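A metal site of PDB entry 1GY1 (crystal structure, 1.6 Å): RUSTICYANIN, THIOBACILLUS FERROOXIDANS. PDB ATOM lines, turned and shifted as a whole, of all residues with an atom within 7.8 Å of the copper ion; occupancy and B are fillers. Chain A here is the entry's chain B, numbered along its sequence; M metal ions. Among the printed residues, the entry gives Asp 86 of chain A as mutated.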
ATOM      1  N   ALA A  44      12.801 -16.827  -2.113  1.00  0.00           N
ATOM      2  CA  ALA A  44      12.321 -17.079  -3.468  1.00  0.00           C
ATOM      3  C   ALA A  44      13.456 -17.700  -4.279  1.00  0.00           C
ATOM      4  O   ALA A  44      14.488 -17.066  -4.518  1.00  0.00           O
ATOM      5  CB  ALA A  44      11.882 -15.765  -4.093  1.00  0.00           C
ATOM      6  N   VAL A  45      13.229 -18.940  -4.701  1.00  0.00           N
ATOM      7  CA  VAL A  45      14.153 -19.710  -5.551  1.00  0.00           C
ATOM      8  C   VAL A  45      15.603 -19.685  -5.059  1.00  0.00           C
ATOM      9  O   VAL A  45      16.470 -19.027  -5.641  1.00  0.00           O
ATOM     10  CB  VAL A  45      14.106 -19.335  -7.036  1.00  0.00           C
ATOM     11  CG1 VAL A  45      14.753 -20.461  -7.874  1.00  0.00           C
ATOM     12  CG2 VAL A  45      12.676 -19.084  -7.479  1.00  0.00           C
ATOM     13  N   PHE A  51      12.556 -23.535 -10.340  1.00  0.00           N
ATOM     14  CA  PHE A  51      11.871 -22.289 -10.606  1.00  0.00           C
ATOM     15  C   PHE A  51      10.483 -22.603 -11.155  1.00  0.00           C
ATOM     16  O   PHE A  51      10.349 -23.472 -12.009  1.00  0.00           O
ATOM     17  CB  PHE A  51      12.642 -21.503 -11.663  1.00  0.00           C
ATOM     18  CG  PHE A  51      11.921 -20.291 -12.154  1.00  0.00           C
ATOM     19  CD1 PHE A  51      10.940 -20.392 -13.127  1.00  0.00           C
ATOM     20  CD2 PHE A  51      12.238 -19.034 -11.667  1.00  0.00           C
ATOM     21  CE1 PHE A  51      10.303 -19.280 -13.592  1.00  0.00           C
ATOM     22  CE2 PHE A  51      11.583 -17.921 -12.128  1.00  0.00           C
ATOM     23  CZ  PHE A  51      10.618 -18.045 -13.084  1.00  0.00           C
ATOM     24  N   PRO A  52       9.434 -21.915 -10.699  1.00  0.00           N
ATOM     25  CA  PRO A  52       9.479 -20.926  -9.620  1.00  0.00           C
ATOM     26  C   PRO A  52       8.955 -21.521  -8.326  1.00  0.00           C
ATOM     27  O   PRO A  52       7.948 -22.214  -8.323  1.00  0.00           O
ATOM     28  CB  PRO A  52       8.511 -19.867 -10.127  1.00  0.00           C
ATOM     29  CG  PRO A  52       7.451 -20.683 -10.896  1.00  0.00           C
ATOM     30  CD  PRO A  52       8.083 -22.027 -11.249  1.00  0.00           C
ATOM     31  N   SER A  53       9.625 -21.240  -7.215  1.00  0.00           N
ATOM     32  CA  SER A  53       9.215 -21.802  -5.950  1.00  0.00           C
ATOM     33  C   SER A  53       9.731 -20.946  -4.821  1.00  0.00           C
ATOM     34  O   SER A  53      10.603 -20.116  -5.033  1.00  0.00           O
ATOM     35  CB  SER A  53       9.773 -23.218  -5.761  1.00  0.00           C
ATOM     36  OG  SER A  53      11.192 -23.195  -5.662  1.00  0.00           O
ATOM     37  N   PHE A  54       9.168 -21.168  -3.634  1.00  0.00           N
ATOM     38  CA  PHE A  54       9.670 -20.607  -2.411  1.00  0.00           C
ATOM     39  C   PHE A  54      10.309 -21.746  -1.633  1.00  0.00           C
ATOM     40  O   PHE A  54       9.827 -22.869  -1.707  1.00  0.00           O
ATOM     41  CB  PHE A  54       8.552 -20.091  -1.528  1.00  0.00           C
ATOM     42  CG  PHE A  54       7.799 -18.916  -2.086  1.00  0.00           C
ATOM     43  CD1 PHE A  54       8.329 -17.650  -2.003  1.00  0.00           C
ATOM     44  CD2 PHE A  54       6.559 -19.077  -2.637  1.00  0.00           C
ATOM     45  CE1 PHE A  54       7.629 -16.554  -2.475  1.00  0.00           C
ATOM     46  CE2 PHE A  54       5.852 -17.989  -3.108  1.00  0.00           C
ATOM     47  CZ  PHE A  54       6.389 -16.727  -3.020  1.00  0.00           C
ATOM     48  N   PHE A  76      11.483 -12.555   4.483  1.00  0.00           N
ATOM     49  CA  PHE A  76      11.401 -13.024   3.105  1.00  0.00           C
ATOM     50  C   PHE A  76      12.604 -12.468   2.345  1.00  0.00           C
ATOM     51  O   PHE A  76      12.859 -11.251   2.372  1.00  0.00           O
ATOM     52  CB  PHE A  76      10.089 -12.617   2.456  1.00  0.00           C
ATOM     53  CG  PHE A  76      10.076 -12.823   0.976  1.00  0.00           C
ATOM     54  CD1 PHE A  76      10.197 -14.085   0.450  1.00  0.00           C
ATOM     55  CD2 PHE A  76       9.937 -11.734   0.112  1.00  0.00           C
ATOM     56  CE1 PHE A  76      10.197 -14.270  -0.916  1.00  0.00           C
ATOM     57  CE2 PHE A  76       9.911 -11.921  -1.240  1.00  0.00           C
ATOM     58  CZ  PHE A  76      10.032 -13.184  -1.766  1.00  0.00           C
ATOM     59  N   ASN A  78      14.709 -12.581  -1.440  1.00  0.00           N
ATOM     60  CA  ASN A  78      14.670 -12.946  -2.839  1.00  0.00           C
ATOM     61  C   ASN A  78      16.073 -13.269  -3.363  1.00  0.00           C
ATOM     62  O   ASN A  78      16.864 -12.376  -3.582  1.00  0.00           O
ATOM     63  CB  ASN A  78      14.061 -11.813  -3.661  1.00  0.00           C
ATOM     64  CG  ASN A  78      14.116 -12.084  -5.139  1.00  0.00           C
ATOM     65  OD1 ASN A  78      14.165 -11.166  -5.971  1.00  0.00           O
ATOM     66  ND2 ASN A  78      14.151 -13.337  -5.468  1.00  0.00           N
ATOM     67  N   ASN A  80      16.631 -14.953  -6.231  1.00  0.00           N
ATOM     68  CA  ASN A  80      16.495 -15.368  -7.622  1.00  0.00           C
ATOM     69  C   ASN A  80      16.846 -14.276  -8.603  1.00  0.00           C
ATOM     70  O   ASN A  80      16.114 -13.314  -8.795  1.00  0.00           O
ATOM     71  CB  ASN A  80      15.075 -15.850  -7.862  1.00  0.00           C
ATOM     72  CG  ASN A  80      14.947 -16.641  -9.146  1.00  0.00           C
ATOM     73  OD1 ASN A  80      15.867 -17.374  -9.563  1.00  0.00           O
ATOM     74  ND2 ASN A  80      13.815 -16.526  -9.766  1.00  0.00           N
ATOM     75  N   PHE A  83      14.507 -11.584 -11.208  1.00  0.00           N
ATOM     76  CA  PHE A  83      13.109 -11.405 -10.837  1.00  0.00           C
ATOM     77  C   PHE A  83      12.973 -10.633  -9.523  1.00  0.00           C
ATOM     78  O   PHE A  83      13.894 -10.601  -8.720  1.00  0.00           O
ATOM     79  CB  PHE A  83      12.441 -12.781 -10.684  1.00  0.00           C
ATOM     80  CG  PHE A  83      12.467 -13.600 -11.950  1.00  0.00           C
ATOM     81  CD1 PHE A  83      13.594 -14.341 -12.274  1.00  0.00           C
ATOM     82  CD2 PHE A  83      11.419 -13.580 -12.821  1.00  0.00           C
ATOM     83  CE1 PHE A  83      13.637 -15.057 -13.453  1.00  0.00           C
ATOM     84  CE2 PHE A  83      11.462 -14.311 -14.014  1.00  0.00           C
ATOM     85  CZ  PHE A  83      12.556 -15.047 -14.308  1.00  0.00           C
ATOM     86  N   GLY A  84      11.807 -10.037  -9.333  1.00  0.00           N
ATOM     87  CA  GLY A  84      11.490  -9.303  -8.113  1.00  0.00           C
ATOM     88  C   GLY A  84      10.297  -9.928  -7.410  1.00  0.00           C
ATOM     89  O   GLY A  84       9.312  -9.266  -7.117  1.00  0.00           O
ATOM     90  N   HIS A  85      10.427 -11.213  -7.084  1.00  0.00           N
ATOM     91  CA  HIS A  85       9.307 -11.939  -6.491  1.00  0.00           C
ATOM     92  C   HIS A  85       8.774 -11.272  -5.233  1.00  0.00           C
ATOM     93  O   HIS A  85       9.517 -10.621  -4.491  1.00  0.00           O
ATOM     94  CB  HIS A  85       9.763 -13.340  -6.078  1.00  0.00           C
ATOM     95  CG  HIS A  85      10.400 -14.141  -7.178  1.00  0.00           C
ATOM     96  ND1 HIS A  85       9.675 -14.793  -8.150  1.00  0.00           N
ATOM     97  CD2 HIS A  85      11.700 -14.438  -7.412  1.00  0.00           C
ATOM     98  CE1 HIS A  85      10.503 -15.462  -8.936  1.00  0.00           C
ATOM     99  NE2 HIS A  85      11.736 -15.253  -8.520  1.00  0.00           N
ATOM    100  N   ASP A  86       7.478 -11.454  -4.997  1.00  0.00           N
ATOM    101  CA  ASP A  86       6.846 -11.009  -3.766  1.00  0.00           C
ATOM    102  C   ASP A  86       6.418 -12.236  -2.953  1.00  0.00           C
ATOM    103  O   ASP A  86       6.522 -13.384  -3.412  1.00  0.00           O
ATOM    104  CB  ASP A  86       5.694 -10.013  -3.973  1.00  0.00           C
ATOM    105  CG  ASP A  86       4.601 -10.492  -4.889  1.00  0.00           C
ATOM    106  OD1 ASP A  86       4.612 -11.651  -5.310  1.00  0.00           O
ATOM    107  OD2 ASP A  86       3.643  -9.724  -5.234  1.00  0.00           O
ATOM    108  N   PHE A  87       5.979 -11.984  -1.735  1.00  0.00           N
ATOM    109  CA  PHE A  87       5.569 -13.054  -0.825  1.00  0.00           C
ATOM    110  C   PHE A  87       4.320 -12.508  -0.156  1.00  0.00           C
ATOM    111  O   PHE A  87       4.406 -11.657   0.746  1.00  0.00           O
ATOM    112  CB  PHE A  87       6.652 -13.346   0.208  1.00  0.00           C
ATOM    113  CG  PHE A  87       6.317 -14.480   1.170  1.00  0.00           C
ATOM    114  CD1 PHE A  87       6.789 -15.754   0.941  1.00  0.00           C
ATOM    115  CD2 PHE A  87       5.561 -14.249   2.299  1.00  0.00           C
ATOM    116  CE1 PHE A  87       6.496 -16.783   1.808  1.00  0.00           C
ATOM    117  CE2 PHE A  87       5.264 -15.274   3.175  1.00  0.00           C
ATOM    118  CZ  PHE A  87       5.735 -16.535   2.939  1.00  0.00           C
ATOM    119  N   PHE A 111       6.748  -6.202  -4.436  1.00  0.00           N
ATOM    120  CA  PHE A 111       7.776  -6.816  -5.248  1.00  0.00           C
ATOM    121  C   PHE A 111       9.169  -6.527  -4.672  1.00  0.00           C
ATOM    122  O   PHE A 111       9.454  -5.406  -4.227  1.00  0.00           O
ATOM    123  CB  PHE A 111       7.647  -6.318  -6.686  1.00  0.00           C
ATOM    124  CG  PHE A 111       6.384  -6.758  -7.323  1.00  0.00           C
ATOM    125  CD1 PHE A 111       6.127  -8.112  -7.485  1.00  0.00           C
ATOM    126  CD2 PHE A 111       5.439  -5.839  -7.702  1.00  0.00           C
ATOM    127  CE1 PHE A 111       4.950  -8.535  -8.070  1.00  0.00           C
ATOM    128  CE2 PHE A 111       4.245  -6.261  -8.283  1.00  0.00           C
ATOM    129  CZ  PHE A 111       4.005  -7.615  -8.450  1.00  0.00           C
ATOM    130  N   VAL A 137       1.987 -16.734  -1.830  1.00  0.00           N
ATOM    131  CA  VAL A 137       1.951 -16.734  -3.267  1.00  0.00           C
ATOM    132  C   VAL A 137       2.784 -15.588  -3.785  1.00  0.00           C
ATOM    133  O   VAL A 137       2.929 -14.589  -3.111  1.00  0.00           O
ATOM    134  CB  VAL A 137       0.490 -16.517  -3.754  1.00  0.00           C
ATOM    135  CG1 VAL A 137       0.357 -16.677  -5.224  1.00  0.00           C
ATOM    136  CG2 VAL A 137      -0.461 -17.474  -3.045  1.00  0.00           C
ATOM    137  N   CYS A 138       3.364 -15.777  -4.963  1.00  0.00           N
ATOM    138  CA  CYS A 138       3.995 -14.705  -5.732  1.00  0.00           C
ATOM    139  C   CYS A 138       3.004 -14.194  -6.788  1.00  0.00           C
ATOM    140  O   CYS A 138       2.308 -14.982  -7.430  1.00  0.00           O
ATOM    141  CB  CYS A 138       5.261 -15.203  -6.418  1.00  0.00           C
ATOM    142  SG  CYS A 138       6.074 -13.923  -7.394  1.00  0.00           S
ATOM    143  N   GLN A 139       2.957 -12.873  -6.965  1.00  0.00           N
ATOM    144  CA  GLN A 139       2.066 -12.260  -7.933  1.00  0.00           C
ATOM    145  C   GLN A 139       2.706 -11.906  -9.273  1.00  0.00           C
ATOM    146  O   GLN A 139       2.016 -11.371 -10.142  1.00  0.00           O
ATOM    147  CB  GLN A 139       1.465 -10.993  -7.350  1.00  0.00           C
ATOM    148  CG  GLN A 139       0.612 -11.223  -6.126  1.00  0.00           C
ATOM    149  CD  GLN A 139      -0.130  -9.979  -5.734  1.00  0.00           C
ATOM    150  OE1 GLN A 139       0.320  -9.227  -4.855  1.00  0.00           O
ATOM    151  NE2 GLN A 139      -1.256  -9.754  -6.358  1.00  0.00           N
ATOM    152  N   ILE A 140       3.986 -12.194  -9.473  1.00  0.00           N
ATOM    153  CA  ILE A 140       4.590 -11.895 -10.776  1.00  0.00           C
ATOM    154  C   ILE A 140       3.807 -12.739 -11.785  1.00  0.00           C
ATOM    155  O   ILE A 140       3.667 -13.945 -11.578  1.00  0.00           O
ATOM    156  CB  ILE A 140       6.074 -12.230 -10.818  1.00  0.00           C
ATOM    157  CG1 ILE A 140       6.869 -11.283  -9.903  1.00  0.00           C
ATOM    158  CG2 ILE A 140       6.571 -12.166 -12.265  1.00  0.00           C
ATOM    159  CD1 ILE A 140       8.336 -11.502  -9.950  1.00  0.00           C
ATOM    160  N   PRO A 141       3.296 -12.123 -12.858  1.00  0.00           N
ATOM    161  CA  PRO A 141       2.434 -12.864 -13.784  1.00  0.00           C
ATOM    162  C   PRO A 141       3.001 -14.194 -14.208  1.00  0.00           C
ATOM    163  O   PRO A 141       4.128 -14.285 -14.726  1.00  0.00           O
ATOM    164  CB  PRO A 141       2.281 -11.907 -14.971  1.00  0.00           C
ATOM    165  CG  PRO A 141       2.374 -10.576 -14.329  1.00  0.00           C
ATOM    166  CD  PRO A 141       3.418 -10.715 -13.257  1.00  0.00           C
ATOM    167  N   GLY A 142       2.213 -15.243 -13.982  1.00  0.00           N
ATOM    168  CA  GLY A 142       2.560 -16.578 -14.400  1.00  0.00           C
ATOM    169  C   GLY A 142       3.213 -17.437 -13.338  1.00  0.00           C
ATOM    170  O   GLY A 142       3.185 -18.653 -13.437  1.00  0.00           O
ATOM    171  N   HIS A 143       3.784 -16.820 -12.305  1.00  0.00           N
ATOM    172  CA  HIS A 143       4.542 -17.611 -11.339  1.00  0.00           C
ATOM    173  C   HIS A 143       3.680 -18.525 -10.483  1.00  0.00           C
ATOM    174  O   HIS A 143       3.982 -19.705 -10.329  1.00  0.00           O
ATOM    175  CB  HIS A 143       5.403 -16.709 -10.458  1.00  0.00           C
ATOM    176  CG  HIS A 143       6.553 -16.105 -11.181  1.00  0.00           C
ATOM    177  ND1 HIS A 143       7.589 -15.457 -10.529  1.00  0.00           N
ATOM    178  CD2 HIS A 143       6.849 -16.054 -12.503  1.00  0.00           C
ATOM    179  CE1 HIS A 143       8.455 -15.029 -11.427  1.00  0.00           C
ATOM    180  NE2 HIS A 143       8.032 -15.367 -12.632  1.00  0.00           N
ATOM    181  N   ALA A 144       2.627 -17.967  -9.893  1.00  0.00           N
ATOM    182  CA  ALA A 144       1.744 -18.768  -9.078  1.00  0.00           C
ATOM    183  C   ALA A 144       1.106 -19.854  -9.929  1.00  0.00           C
ATOM    184  O   ALA A 144       0.953 -20.986  -9.489  1.00  0.00           O
ATOM    185  CB  ALA A 144       0.705 -17.904  -8.443  1.00  0.00           C
ATOM    186  N   MET A 148       4.447 -21.335  -7.971  1.00  0.00           N
ATOM    187  CA  MET A 148       5.105 -20.532  -6.946  1.00  0.00           C
ATOM    188  C   MET A 148       4.111 -20.144  -5.851  1.00  0.00           C
ATOM    189  O   MET A 148       3.673 -18.996  -5.760  1.00  0.00           O
ATOM    190  CB  MET A 148       5.777 -19.282  -7.536  1.00  0.00           C
ATOM    191  CG  MET A 148       6.718 -18.618  -6.538  1.00  0.00           C
ATOM    192  SD  MET A 148       7.912 -17.573  -7.342  1.00  0.00           S
ATOM    193  CE  MET A 148       8.902 -17.085  -5.925  1.00  0.00           C
HETATM  194 CU    CU M   1       7.644 -15.037  -8.481  1.00  0.00          CU
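The side-chain amide nitrogen (ND2) of Asn 80 lies within hydrogen-bond range of a ring nitrogen (NE2) of His 85, at 2.7 Å. SG of Cys 138 sits close to N of Ile 140, 3.4 Å away. The side-chain carboxylate (OD1) of Asp 86 sits close to the side-chain sulfur (SG) of Cys 138, at 3.4 Å.
Merely in contact with the copper ion: Ile 140. Five residues have an atom within 4 Å of the copper ion: His 85, Cys 138, Ile 140, His 143 and Met 148. Along chain A the residues within 4 Å of the copper ion span positions 85 to 148. The nearest printed residue that does not touch the copper ion is Asp 86 (5.0 Å).
ND1 of His 85 binds the copper ion (2.1 Å). ND1 of His 143 is bound to the copper ion (2.1 Å). SG of Cys 138 is bound to the copper ion, 2.2 Å away. SD of Met 148 binds the copper ion (2.8 Å). The copper ion has four donor atoms within binding distance.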
